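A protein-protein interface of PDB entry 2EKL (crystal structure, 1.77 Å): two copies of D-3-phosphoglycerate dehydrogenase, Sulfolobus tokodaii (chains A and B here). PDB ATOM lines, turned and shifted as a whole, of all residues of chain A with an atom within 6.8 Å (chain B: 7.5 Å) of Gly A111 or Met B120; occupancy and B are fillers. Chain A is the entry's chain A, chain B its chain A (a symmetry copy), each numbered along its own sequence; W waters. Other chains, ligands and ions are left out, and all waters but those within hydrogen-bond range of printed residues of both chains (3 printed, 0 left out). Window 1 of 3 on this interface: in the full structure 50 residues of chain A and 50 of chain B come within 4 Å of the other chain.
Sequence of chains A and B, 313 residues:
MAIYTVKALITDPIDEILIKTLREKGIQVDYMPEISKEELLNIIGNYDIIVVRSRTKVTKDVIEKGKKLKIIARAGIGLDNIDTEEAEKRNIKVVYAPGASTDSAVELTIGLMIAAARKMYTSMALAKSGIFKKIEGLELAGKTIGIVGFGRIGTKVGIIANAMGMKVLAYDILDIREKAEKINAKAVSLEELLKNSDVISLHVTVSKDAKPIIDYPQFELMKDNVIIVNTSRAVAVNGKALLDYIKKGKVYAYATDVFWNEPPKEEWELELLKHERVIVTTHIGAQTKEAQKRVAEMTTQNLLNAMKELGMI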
ATOM      1  N   VAL A 106     -13.923  16.922 -10.658  1.00  0.00           N
ATOM      2  CA  VAL A 106     -13.527  16.870  -9.251  1.00  0.00           C
ATOM      3  C   VAL A 106     -14.672  16.329  -8.397  1.00  0.00           C
ATOM      4  O   VAL A 106     -14.483  15.462  -7.539  1.00  0.00           O
ATOM      5  CB  VAL A 106     -13.167  18.285  -8.718  1.00  0.00           C
ATOM      6  CG1 VAL A 106     -13.065  18.261  -7.201  1.00  0.00           C
ATOM      7  CG2 VAL A 106     -11.852  18.763  -9.332  1.00  0.00           C
ATOM      8  N   GLU A 107     -15.865  16.859  -8.634  1.00  0.00           N
ATOM      9  CA  GLU A 107     -17.032  16.447  -7.878  1.00  0.00           C
ATOM     10  C   GLU A 107     -17.373  14.980  -8.104  1.00  0.00           C
ATOM     11  O   GLU A 107     -17.684  14.261  -7.153  1.00  0.00           O
ATOM     12  CB  GLU A 107     -18.213  17.363  -8.224  1.00  0.00           C
ATOM     13  CG  GLU A 107     -18.060  18.755  -7.600  1.00  0.00           C
ATOM     14  CD  GLU A 107     -18.794  19.847  -8.357  1.00  0.00           C
ATOM     15  OE1 GLU A 107     -19.789  19.545  -9.049  1.00  0.00           O
ATOM     16  OE2 GLU A 107     -18.380  21.021  -8.242  1.00  0.00           O
ATOM     17  N   LEU A 108     -17.303  14.525  -9.351  1.00  0.00           N
ATOM     18  CA  LEU A 108     -17.608  13.127  -9.627  1.00  0.00           C
ATOM     19  C   LEU A 108     -16.583  12.237  -8.933  1.00  0.00           C
ATOM     20  O   LEU A 108     -16.916  11.151  -8.464  1.00  0.00           O
ATOM     21  CB  LEU A 108     -17.594  12.842 -11.131  1.00  0.00           C
ATOM     22  CG  LEU A 108     -17.991  11.409 -11.512  1.00  0.00           C
ATOM     23  CD1 LEU A 108     -19.445  11.161 -11.124  1.00  0.00           C
ATOM     24  CD2 LEU A 108     -17.800  11.194 -13.010  1.00  0.00           C
ATOM     25  N   THR A 109     -15.336  12.701  -8.860  1.00  0.00           N
ATOM     26  CA  THR A 109     -14.276  11.925  -8.210  1.00  0.00           C
ATOM     27  C   THR A 109     -14.623  11.684  -6.743  1.00  0.00           C
ATOM     28  O   THR A 109     -14.547  10.554  -6.252  1.00  0.00           O
ATOM     29  CB  THR A 109     -12.912  12.650  -8.285  1.00  0.00           C
ATOM     30  OG1 THR A 109     -12.547  12.847  -9.657  1.00  0.00           O
ATOM     31  CG2 THR A 109     -11.827  11.821  -7.590  1.00  0.00           C
ATOM     32  N   ILE A 110     -14.997  12.753  -6.042  1.00  0.00           N
ATOM     33  CA  ILE A 110     -15.367  12.654  -4.631  1.00  0.00           C
ATOM     34  C   ILE A 110     -16.598  11.762  -4.488  1.00  0.00           C
ATOM     35  O   ILE A 110     -16.695  10.953  -3.557  1.00  0.00           O
ATOM     36  CB  ILE A 110     -15.682  14.054  -4.034  1.00  0.00           C
ATOM     37  CG1 ILE A 110     -14.419  14.925  -4.056  1.00  0.00           C
ATOM     38  CG2 ILE A 110     -16.226  13.915  -2.609  1.00  0.00           C
ATOM     39  CD1 ILE A 110     -13.246  14.357  -3.265  1.00  0.00           C
ATOM     40  N   GLY A 111     -17.540  11.910  -5.413  1.00  0.00           N
ATOM     41  CA  GLY A 111     -18.745  11.100  -5.364  1.00  0.00           C
ATOM     42  C   GLY A 111     -18.421   9.621  -5.522  1.00  0.00           C
ATOM     43  O   GLY A 111     -18.970   8.781  -4.808  1.00  0.00           O
ATOM     44  N   LEU A 112     -17.543   9.298  -6.468  1.00  0.00           N
ATOM     45  CA  LEU A 112     -17.147   7.908  -6.705  1.00  0.00           C
ATOM     46  C   LEU A 112     -16.410   7.335  -5.497  1.00  0.00           C
ATOM     47  O   LEU A 112     -16.645   6.189  -5.095  1.00  0.00           O
ATOM     48  CB  LEU A 112     -16.258   7.812  -7.956  1.00  0.00           C
ATOM     49  CG  LEU A 112     -16.979   7.913  -9.304  1.00  0.00           C
ATOM     50  CD1 LEU A 112     -15.969   8.010 -10.445  1.00  0.00           C
ATOM     51  CD2 LEU A 112     -17.868   6.685  -9.485  1.00  0.00           C
ATOM     52  N   MET A 113     -15.529   8.132  -4.903  1.00  0.00           N
ATOM     53  CA  MET A 113     -14.777   7.681  -3.734  1.00  0.00           C
ATOM     54  C   MET A 113     -15.724   7.278  -2.600  1.00  0.00           C
ATOM     55  O   MET A 113     -15.569   6.217  -1.993  1.00  0.00           O
ATOM     56  CB  MET A 113     -13.835   8.789  -3.252  1.00  0.00           C
ATOM     57  CG  MET A 113     -13.092   8.444  -1.965  1.00  0.00           C
ATOM     58  SD  MET A 113     -11.954   9.753  -1.437  1.00  0.00           S
ATOM     59  CE  MET A 113     -13.105  11.019  -0.906  1.00  0.00           C
ATOM     60  N   ILE A 114     -16.708   8.124  -2.322  1.00  0.00           N
ATOM     61  CA  ILE A 114     -17.656   7.841  -1.252  1.00  0.00           C
ATOM     62  C   ILE A 114     -18.576   6.682  -1.626  1.00  0.00           C
ATOM     63  O   ILE A 114     -18.862   5.825  -0.794  1.00  0.00           O
ATOM     64  CB  ILE A 114     -18.497   9.091  -0.916  1.00  0.00           C
ATOM     65  CG1 ILE A 114     -17.571  10.205  -0.415  1.00  0.00           C
ATOM     66  CG2 ILE A 114     -19.527   8.759   0.157  1.00  0.00           C
ATOM     67  CD1 ILE A 114     -18.244  11.570  -0.303  1.00  0.00           C
ATOM     68  N   ALA A 115     -19.031   6.650  -2.874  1.00  0.00           N
ATOM     69  CA  ALA A 115     -19.916   5.569  -3.314  1.00  0.00           C
ATOM     70  C   ALA A 115     -19.209   4.225  -3.179  1.00  0.00           C
ATOM     71  O   ALA A 115     -19.817   3.235  -2.770  1.00  0.00           O
ATOM     72  CB  ALA A 115     -20.352   5.795  -4.756  1.00  0.00           C
ATOM     73  N   ALA A 116     -17.921   4.199  -3.506  1.00  0.00           N
ATOM     74  CA  ALA A 116     -17.127   2.969  -3.414  1.00  0.00           C
ATOM     75  C   ALA A 116     -16.910   2.561  -1.959  1.00  0.00           C
ATOM     76  O   ALA A 116     -17.056   1.392  -1.594  1.00  0.00           O
ATOM     77  CB  ALA A 116     -15.777   3.171  -4.098  1.00  0.00           C
ATOM     78  N   MET A 120     -22.667   2.483  -1.965  1.00  0.00           N
ATOM     79  CA  MET A 120     -23.909   3.203  -2.197  1.00  0.00           C
ATOM     80  C   MET A 120     -24.764   2.599  -3.305  1.00  0.00           C
ATOM     81  O   MET A 120     -25.987   2.575  -3.199  1.00  0.00           O
ATOM     82  CB  MET A 120     -23.618   4.677  -2.504  1.00  0.00           C
ATOM     83  CG  MET A 120     -23.140   5.453  -1.290  1.00  0.00           C
ATOM     84  SD  MET A 120     -22.862   7.207  -1.614  1.00  0.00           S
ATOM     85  CE  MET A 120     -24.518   7.795  -1.719  1.00  0.00           C
ATOM     86  N   TYR A 121     -24.129   2.116  -4.368  1.00  0.00           N
ATOM     87  CA  TYR A 121     -24.885   1.535  -5.471  1.00  0.00           C
ATOM     88  C   TYR A 121     -25.711   0.350  -4.995  1.00  0.00           C
ATOM     89  O   TYR A 121     -26.899   0.249  -5.290  1.00  0.00           O
ATOM     90  CB  TYR A 121     -23.953   1.074  -6.589  1.00  0.00           C
ATOM     91  CG  TYR A 121     -24.703   0.430  -7.732  1.00  0.00           C
ATOM     92  CD1 TYR A 121     -25.617   1.162  -8.489  1.00  0.00           C
ATOM     93  CD2 TYR A 121     -24.528  -0.919  -8.032  1.00  0.00           C
ATOM     94  CE1 TYR A 121     -26.342   0.562  -9.521  1.00  0.00           C
ATOM     95  CE2 TYR A 121     -25.246  -1.528  -9.062  1.00  0.00           C
ATOM     96  CZ  TYR A 121     -26.147  -0.783  -9.799  1.00  0.00           C
ATOM     97  OH  TYR A 121     -26.845  -1.383 -10.824  1.00  0.00           O
ATOM     98  N   MET A 124     -28.600   1.607  -2.906  1.00  0.00           N
ATOM     99  CA  MET A 124     -29.632   2.278  -3.686  1.00  0.00           C
ATOM    100  C   MET A 124     -30.449   1.286  -4.504  1.00  0.00           C
ATOM    101  O   MET A 124     -31.662   1.455  -4.668  1.00  0.00           O
ATOM    102  CB  MET A 124     -29.015   3.330  -4.608  1.00  0.00           C
ATOM    103  CG  MET A 124     -28.324   4.463  -3.871  1.00  0.00           C
ATOM    104  SD  MET A 124     -27.613   5.647  -5.031  1.00  0.00           S
ATOM    105  CE  MET A 124     -26.148   4.825  -5.487  1.00  0.00           C
ATOM    106  N   ALA A 255     -13.348   2.396  -8.227  1.00  0.00           N
ATOM    107  CA  ALA A 255     -14.435   3.270  -8.670  1.00  0.00           C
ATOM    108  C   ALA A 255     -13.910   4.081  -9.840  1.00  0.00           C
ATOM    109  O   ALA A 255     -12.936   4.815  -9.696  1.00  0.00           O
ATOM    110  CB  ALA A 255     -14.863   4.192  -7.531  1.00  0.00           C
ATOM    111  N   ILE A 279     -17.079  -0.206  -9.263  1.00  0.00           N
ATOM    112  CA  ILE A 279     -18.110   0.826  -9.401  1.00  0.00           C
ATOM    113  C   ILE A 279     -17.782   1.621 -10.662  1.00  0.00           C
ATOM    114  O   ILE A 279     -16.666   2.118 -10.809  1.00  0.00           O
ATOM    115  CB  ILE A 279     -18.112   1.792  -8.178  1.00  0.00           C
ATOM    116  CG1 ILE A 279     -18.576   1.058  -6.915  1.00  0.00           C
ATOM    117  CG2 ILE A 279     -19.031   2.975  -8.449  1.00  0.00           C
ATOM    118  CD1 ILE A 279     -17.555   0.106  -6.322  1.00  0.00           C
ATOM    119  N   VAL A 280     -18.751   1.755 -11.560  1.00  0.00           N
ATOM    120  CA  VAL A 280     -18.506   2.454 -12.813  1.00  0.00           C
ATOM    121  C   VAL A 280     -19.577   3.450 -13.246  1.00  0.00           C
ATOM    122  O   VAL A 280     -20.771   3.156 -13.195  1.00  0.00           O
ATOM    123  CB  VAL A 280     -18.357   1.440 -13.992  1.00  0.00           C
ATOM    124  CG1 VAL A 280     -17.925   2.176 -15.261  1.00  0.00           C
ATOM    125  CG2 VAL A 280     -17.366   0.341 -13.633  1.00  0.00           C
ATOM    126  N   THR A 281     -19.145   4.637 -13.662  1.00  0.00           N
ATOM    127  CA  THR A 281     -20.075   5.616 -14.202  1.00  0.00           C
ATOM    128  C   THR A 281     -19.706   5.679 -15.682  1.00  0.00           C
ATOM    129  O   THR A 281     -18.569   5.384 -16.065  1.00  0.00           O
ATOM    130  CB  THR A 281     -19.978   7.001 -13.517  1.00  0.00           C
ATOM    131  OG1 THR A 281     -18.609   7.364 -13.319  1.00  0.00           O
ATOM    132  CG2 THR A 281     -20.703   6.961 -12.165  1.00  0.00           C
ATOM    133  N   ILE A 284     -19.147  10.315 -17.384  1.00  0.00           N
ATOM    134  CA  ILE A 284     -19.947  11.519 -17.201  1.00  0.00           C
ATOM    135  C   ILE A 284     -19.207  12.633 -16.464  1.00  0.00           C
ATOM    136  O   ILE A 284     -19.823  13.605 -16.035  1.00  0.00           O
ATOM    137  CB  ILE A 284     -21.242  11.195 -16.419  1.00  0.00           C
ATOM    138  CG1 ILE A 284     -20.895  10.582 -15.058  1.00  0.00           C
ATOM    139  CG2 ILE A 284     -22.104  10.216 -17.227  1.00  0.00           C
ATOM    140  CD1 ILE A 284     -22.103  10.307 -14.175  1.00  0.00           C
ATOM    141  N   ILE B 110     -22.426  14.020   1.752  1.00  0.00           N
ATOM    142  CA  ILE B 110     -21.725  14.555   0.586  1.00  0.00           C
ATOM    143  C   ILE B 110     -21.896  13.601  -0.594  1.00  0.00           C
ATOM    144  O   ILE B 110     -22.088  14.031  -1.739  1.00  0.00           O
ATOM    145  CB  ILE B 110     -20.209  14.736   0.876  1.00  0.00           C
ATOM    146  CG1 ILE B 110     -20.012  15.786   1.977  1.00  0.00           C
ATOM    147  CG2 ILE B 110     -19.465  15.137  -0.401  1.00  0.00           C
ATOM    148  CD1 ILE B 110     -20.568  17.165   1.642  1.00  0.00           C
ATOM    149  N   GLY B 111     -21.828  12.305  -0.314  1.00  0.00           N
ATOM    150  CA  GLY B 111     -21.986  11.321  -1.371  1.00  0.00           C
ATOM    151  C   GLY B 111     -23.371  11.403  -1.998  1.00  0.00           C
ATOM    152  O   GLY B 111     -23.510  11.339  -3.219  1.00  0.00           O
ATOM    153  N   LEU B 112     -24.399  11.528  -1.162  1.00  0.00           N
ATOM    154  CA  LEU B 112     -25.776  11.627  -1.650  1.00  0.00           C
ATOM    155  C   LEU B 112     -25.979  12.904  -2.463  1.00  0.00           C
ATOM    156  O   LEU B 112     -26.627  12.888  -3.517  1.00  0.00           O
ATOM    157  CB  LEU B 112     -26.764  11.594  -0.472  1.00  0.00           C
ATOM    158  CG  LEU B 112     -27.010  10.220   0.161  1.00  0.00           C
ATOM    159  CD1 LEU B 112     -27.841  10.360   1.435  1.00  0.00           C
ATOM    160  CD2 LEU B 112     -27.731   9.330  -0.848  1.00  0.00           C
ATOM    161  N   MET B 113     -25.415  14.008  -1.989  1.00  0.00           N
ATOM    162  CA  MET B 113     -25.542  15.280  -2.697  1.00  0.00           C
ATOM    163  C   MET B 113     -24.986  15.170  -4.119  1.00  0.00           C
ATOM    164  O   MET B 113     -25.624  15.595  -5.084  1.00  0.00           O
ATOM    165  CB  MET B 113     -24.803  16.385  -1.937  1.00  0.00           C
ATOM    166  CG  MET B 113     -24.790  17.726  -2.664  1.00  0.00           C
ATOM    167  SD  MET B 113     -23.943  19.027  -1.726  1.00  0.00           S
ATOM    168  CE  MET B 113     -22.239  18.490  -1.848  1.00  0.00           C
ATOM    169  N   ILE B 114     -23.798  14.593  -4.246  1.00  0.00           N
ATOM    170  CA  ILE B 114     -23.173  14.451  -5.556  1.00  0.00           C
ATOM    171  C   ILE B 114     -23.913  13.424  -6.409  1.00  0.00           C
ATOM    172  O   ILE B 114     -24.114  13.640  -7.601  1.00  0.00           O
ATOM    173  CB  ILE B 114     -21.690  14.045  -5.417  1.00  0.00           C
ATOM    174  CG1 ILE B 114     -20.930  15.149  -4.672  1.00  0.00           C
ATOM    175  CG2 ILE B 114     -21.071  13.836  -6.794  1.00  0.00           C
ATOM    176  CD1 ILE B 114     -19.521  14.752  -4.240  1.00  0.00           C
ATOM    177  N   ALA B 115     -24.324  12.317  -5.801  1.00  0.00           N
ATOM    178  CA  ALA B 115     -25.046  11.284  -6.548  1.00  0.00           C
ATOM    179  C   ALA B 115     -26.340  11.856  -7.117  1.00  0.00           C
ATOM    180  O   ALA B 115     -26.714  11.555  -8.251  1.00  0.00           O
ATOM    181  CB  ALA B 115     -25.345  10.091  -5.649  1.00  0.00           C
ATOM    182  N   ALA B 116     -27.010  12.695  -6.333  1.00  0.00           N
ATOM    183  CA  ALA B 116     -28.266  13.317  -6.766  1.00  0.00           C
ATOM    184  C   ALA B 116     -28.022  14.332  -7.881  1.00  0.00           C
ATOM    185  O   ALA B 116     -28.739  14.365  -8.884  1.00  0.00           O
ATOM    186  CB  ALA B 116     -28.939  14.007  -5.581  1.00  0.00           C
ATOM    187  N   ALA B 117     -27.014  15.171  -7.690  1.00  0.00           N
ATOM    188  CA  ALA B 117     -26.674  16.192  -8.667  1.00  0.00           C
ATOM    189  C   ALA B 117     -26.233  15.601 -10.001  1.00  0.00           C
ATOM    190  O   ALA B 117     -26.496  16.176 -11.058  1.00  0.00           O
ATOM    191  CB  ALA B 117     -25.565  17.087  -8.111  1.00  0.00           C
ATOM    192  N   ARG B 118     -25.594  14.437  -9.959  1.00  0.00           N
ATOM    193  CA  ARG B 118     -25.064  13.840 -11.176  1.00  0.00           C
ATOM    194  C   ARG B 118     -25.747  12.576 -11.677  1.00  0.00           C
ATOM    195  O   ARG B 118     -25.247  11.935 -12.603  1.00  0.00           O
ATOM    196  CB  ARG B 118     -23.570  13.575 -10.971  1.00  0.00           C
ATOM    197  CG  ARG B 118     -22.799  14.852 -10.666  1.00  0.00           C
ATOM    198  CD  ARG B 118     -22.738  15.739 -11.904  1.00  0.00           C
ATOM    199  NE  ARG B 118     -21.732  15.261 -12.853  1.00  0.00           N
ATOM    200  CZ  ARG B 118     -20.429  15.508 -12.747  1.00  0.00           C
ATOM    201  NH1 ARG B 118     -19.964  16.234 -11.732  1.00  0.00           N
ATOM    202  NH2 ARG B 118     -19.587  15.030 -13.656  1.00  0.00           N
ATOM    203  N   LYS B 119     -26.880  12.229 -11.076  1.00  0.00           N
ATOM    204  CA  LYS B 119     -27.624  11.032 -11.468  1.00  0.00           C
ATOM    205  C   LYS B 119     -26.682   9.844 -11.539  1.00  0.00           C
ATOM    206  O   LYS B 119     -26.709   9.066 -12.494  1.00  0.00           O
ATOM    207  CB  LYS B 119     -28.290  11.253 -12.830  1.00  0.00           C
ATOM    208  CG  LYS B 119     -29.222  12.447 -12.833  1.00  0.00           C
ATOM    209  CD  LYS B 119     -29.783  12.733 -14.210  1.00  0.00           C
ATOM    210  CE  LYS B 119     -30.627  13.994 -14.192  1.00  0.00           C
ATOM    211  NZ  LYS B 119     -31.136  14.340 -15.549  1.00  0.00           N
ATOM    212  N   MET B 120     -25.843   9.701 -10.519  1.00  0.00           N
ATOM    213  CA  MET B 120     -24.886   8.606 -10.497  1.00  0.00           C
ATOM    214  C   MET B 120     -25.537   7.229 -10.502  1.00  0.00           C
ATOM    215  O   MET B 120     -25.032   6.309 -11.139  1.00  0.00           O
ATOM    216  CB  MET B 120     -23.954   8.742  -9.287  1.00  0.00           C
ATOM    217  CG  MET B 120     -22.970   9.890  -9.420  1.00  0.00           C
ATOM    218  SD  MET B 120     -21.815  10.019  -8.038  1.00  0.00           S
ATOM    219  CE  MET B 120     -20.746   8.662  -8.366  1.00  0.00           C
ATOM    220  N   TYR B 121     -26.652   7.081  -9.794  1.00  0.00           N
ATOM    221  CA  TYR B 121     -27.321   5.787  -9.744  1.00  0.00           C
ATOM    222  C   TYR B 121     -27.736   5.338 -11.138  1.00  0.00           C
ATOM    223  O   TYR B 121     -27.487   4.204 -11.537  1.00  0.00           O
ATOM    224  CB  TYR B 121     -28.558   5.845  -8.852  1.00  0.00           C
ATOM    225  CG  TYR B 121     -29.299   4.528  -8.811  1.00  0.00           C
ATOM    226  CD1 TYR B 121     -28.696   3.387  -8.284  1.00  0.00           C
ATOM    227  CD2 TYR B 121     -30.585   4.415  -9.332  1.00  0.00           C
ATOM    228  CE1 TYR B 121     -29.361   2.158  -8.278  1.00  0.00           C
ATOM    229  CE2 TYR B 121     -31.258   3.192  -9.330  1.00  0.00           C
ATOM    230  CZ  TYR B 121     -30.642   2.074  -8.804  1.00  0.00           C
ATOM    231  OH  TYR B 121     -31.313   0.871  -8.791  1.00  0.00           O
ATOM    232  N   THR B 122     -28.378   6.237 -11.869  1.00  0.00           N
ATOM    233  CA  THR B 122     -28.837   5.931 -13.214  1.00  0.00           C
ATOM    234  C   THR B 122     -27.662   5.501 -14.090  1.00  0.00           C
ATOM    235  O   THR B 122     -27.750   4.515 -14.826  1.00  0.00           O
ATOM    236  CB  THR B 122     -29.531   7.151 -13.842  1.00  0.00           C
ATOM    237  OG1 THR B 122     -30.639   7.545 -13.020  1.00  0.00           O
ATOM    238  CG2 THR B 122     -30.034   6.818 -15.243  1.00  0.00           C
ATOM    239  N   SER B 123     -26.561   6.238 -13.989  1.00  0.00           N
ATOM    240  CA  SER B 123     -25.360   5.952 -14.767  1.00  0.00           C
ATOM    241  C   SER B 123     -24.744   4.606 -14.387  1.00  0.00           C
ATOM    242  O   SER B 123     -24.355   3.824 -15.259  1.00  0.00           O
ATOM    243  CB  SER B 123     -24.330   7.070 -14.557  1.00  0.00           C
ATOM    244  OG  SER B 123     -23.206   6.922 -15.414  1.00  0.00           O
ATOM    245  N   MET B 124     -24.658   4.330 -13.087  1.00  0.00           N
ATOM    246  CA  MET B 124     -24.069   3.076 -12.634  1.00  0.00           C
ATOM    247  C   MET B 124     -24.916   1.879 -13.046  1.00  0.00           C
ATOM    248  O   MET B 124     -24.381   0.817 -13.384  1.00  0.00           O
ATOM    249  CB  MET B 124     -23.880   3.084 -11.117  1.00  0.00           C
ATOM    250  CG  MET B 124     -22.908   4.140 -10.625  1.00  0.00           C
ATOM    251  SD  MET B 124     -22.758   4.089  -8.827  1.00  0.00           S
ATOM    252  CE  MET B 124     -24.194   4.948  -8.351  1.00  0.00           C
ATOM    253  N   ALA B 125     -26.234   2.049 -13.024  1.00  0.00           N
ATOM    254  CA  ALA B 125     -27.132   0.966 -13.418  1.00  0.00           C
ATOM    255  C   ALA B 125     -26.929   0.688 -14.904  1.00  0.00           C
ATOM    256  O   ALA B 125     -26.860  -0.468 -15.331  1.00  0.00           O
ATOM    257  CB  ALA B 125     -28.577   1.354 -13.147  1.00  0.00           C
ATOM    258  N   LEU B 126     -26.837   1.754 -15.692  1.00  0.00           N
ATOM    259  CA  LEU B 126     -26.620   1.615 -17.122  1.00  0.00           C
ATOM    260  C   LEU B 126     -25.312   0.879 -17.383  1.00  0.00           C
ATOM    261  O   LEU B 126     -25.276  -0.082 -18.146  1.00  0.00           O
ATOM    262  CB  LEU B 126     -26.590   2.991 -17.789  1.00  0.00           C
ATOM    263  CG  LEU B 126     -27.966   3.624 -18.006  1.00  0.00           C
ATOM    264  CD1 LEU B 126     -27.833   5.106 -18.294  1.00  0.00           C
ATOM    265  CD2 LEU B 126     -28.660   2.907 -19.159  1.00  0.00           C
ATOM    266  N   ILE B 135     -24.982  10.614 -19.188  1.00  0.00           N
ATOM    267  CA  ILE B 135     -26.135  11.270 -18.577  1.00  0.00           C
ATOM    268  C   ILE B 135     -25.655  12.605 -18.009  1.00  0.00           C
ATOM    269  O   ILE B 135     -24.615  12.663 -17.358  1.00  0.00           O
ATOM    270  CB  ILE B 135     -26.723  10.402 -17.437  1.00  0.00           C
ATOM    271  CG1 ILE B 135     -27.829  11.163 -16.704  1.00  0.00           C
ATOM    272  CG2 ILE B 135     -25.626   9.990 -16.483  1.00  0.00           C
ATOM    273  CD1 ILE B 135     -29.032  11.474 -17.570  1.00  0.00           C
ATOM    274  N   MET B 164     -15.466  22.619  -1.505  1.00  0.00           N
ATOM    275  CA  MET B 164     -15.905  22.264  -2.849  1.00  0.00           C
ATOM    276  C   MET B 164     -16.245  23.533  -3.634  1.00  0.00           C
ATOM    277  O   MET B 164     -16.740  23.468  -4.756  1.00  0.00           O
ATOM    278  CB  MET B 164     -17.134  21.347  -2.781  1.00  0.00           C
ATOM    279  CG  MET B 164     -16.844  19.982  -2.160  1.00  0.00           C
ATOM    280  SD  MET B 164     -18.346  18.974  -1.980  1.00  0.00           S
ATOM    281  CE  MET B 164     -18.823  18.752  -3.685  1.00  0.00           C
ATOM    282  N   ILE B 279     -33.472   9.706  -4.729  1.00  0.00           N
ATOM    283  CA  ILE B 279     -32.304   8.854  -4.489  1.00  0.00           C
ATOM    284  C   ILE B 279     -32.361   8.415  -3.029  1.00  0.00           C
ATOM    285  O   ILE B 279     -32.464   9.251  -2.133  1.00  0.00           O
ATOM    286  CB  ILE B 279     -30.976   9.632  -4.733  1.00  0.00           C
ATOM    287  CG1 ILE B 279     -30.814   9.968  -6.220  1.00  0.00           C
ATOM    288  CG2 ILE B 279     -29.789   8.801  -4.264  1.00  0.00           C
ATOM    289  CD1 ILE B 279     -31.709  11.087  -6.719  1.00  0.00           C
HETATM  290  O   HOH W   1     -21.494  17.649  -9.635  1.00  0.00           O
HETATM  291  O   HOH W   2     -21.611   0.660 -12.326  1.00  0.00           O
HETATM  292  O   HOH W   3     -16.340  21.372  -6.428  1.00  0.00           O
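Gly A111 touches just these residues of chain B: Ile B114 (3.7 Å) and Met B120 (3.8 Å). Met B120 touches three residues of chain A. Printed residues of chain A within 4 Å of Arg B118: Leu A108 (3.9 Å) and Ile A284 (2.8 Å). Printed residues of chain A within 4 Å of Ala B125: Tyr A121. Of the printed residues of chain B, Met A120 touches Gly B111 (3.8 Å) and Leu B112 (3.7 Å). Val A106 touches none of the printed residues of chain B. The nearest residue of chain B that does not touch Gly A111 is Gly B111 (5.1 Å). The nearest printed residue of chain A that does not touch Ile B114 is Leu A108 (4.5 Å).
Ile A110 touches Ile B114, and with the chains exchanged Ile A114 touches Ile B110. Gly A111 touches Met B120, and with the chains exchanged Met A120 touches Gly B111. Leu A112 touches Met B120, and with the chains exchanged Met A120 touches Leu B112. Met A124 touches its own counterpart, Met B124. 11 positions are printed for both chains.
Leu A108 touches Met B120 (CD1 to CE, 3.9 Å). Met B120 touches Gly A111. Leu A112 touches Met B120. Ile B110 touches Ile A114. CE of Met A120 touches C of Gly B111, at 3.8 Å. Met A120 touches Leu B112 (CE to CD2, 3.7 Å). Tyr A121 touches Met B124 (CD1 to CB, 3.7 Å). Ala B125 touches Tyr A121 (CA to OH, 3.5 Å). Met B124 touches Ile A279. CG of Met B124 touches CG2 of Thr A281 (3.9 Å).
The backbone NH (N) of Met B120 lies within hydrogen-bond range of the backbone carbonyl oxygen (O) of Ala B115 (3.1 Å). N of Met A120 lies within hydrogen-bond range of O of Ala A115, at 3.1 Å.
Printed residues of chain B that touch a printed residue of chain A: Ile B110, Gly B111, Leu B112, Ile B114, Arg B118, Met B120, Tyr B121, Ser B123, Met B124, Ala B125, Ile B135, Met B164 and Ile B279. Hydrophobic or aromatic side chains of chain B that line the printed part of chain A: Ile B110, Leu B112, Ile B114, Met B120, Tyr B121, Met B124, Ala B125, Ile B135, Met B164 and Ile B279. Of the 19 printed residues of chain A, 13 touch a printed residue of chain B. Hydrophobic or aromatic side chains of chain A within 4 Å of the printed part of chain B: Leu A108, Ile A110, Leu A112, Ile A114, Met A120, Tyr A121, Met A124, Ile A279 and Ile A284. Among the printed residues, 25 pairs touch across the chains. Among the printed residues, no Asp or Glu carboxylate lies within 4 Å of a Lys or Arg side-chain nitrogen of the other chain.
Water W1 lies within hydrogen-bond range of OE1 of Glu A107 (2.6 Å) and NH1 of Arg B118 (3.0 Å). Water W3 lies within hydrogen-bond range of the backbone carbonyl oxygen of Met B164 (2.7 Å) and the side-chain carboxylate of Glu A107 (2.8 Å). Water W2 lies within hydrogen-bond range of the backbone carbonyl oxygen of Val A280 and the backbone carbonyl oxygen of Met B124.
The backbone carbonyl oxygen (O) of Ile A284 sits at hydrogen-bond distance from the guanidinium group (NH2) of Arg B118 (2.8 Å).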
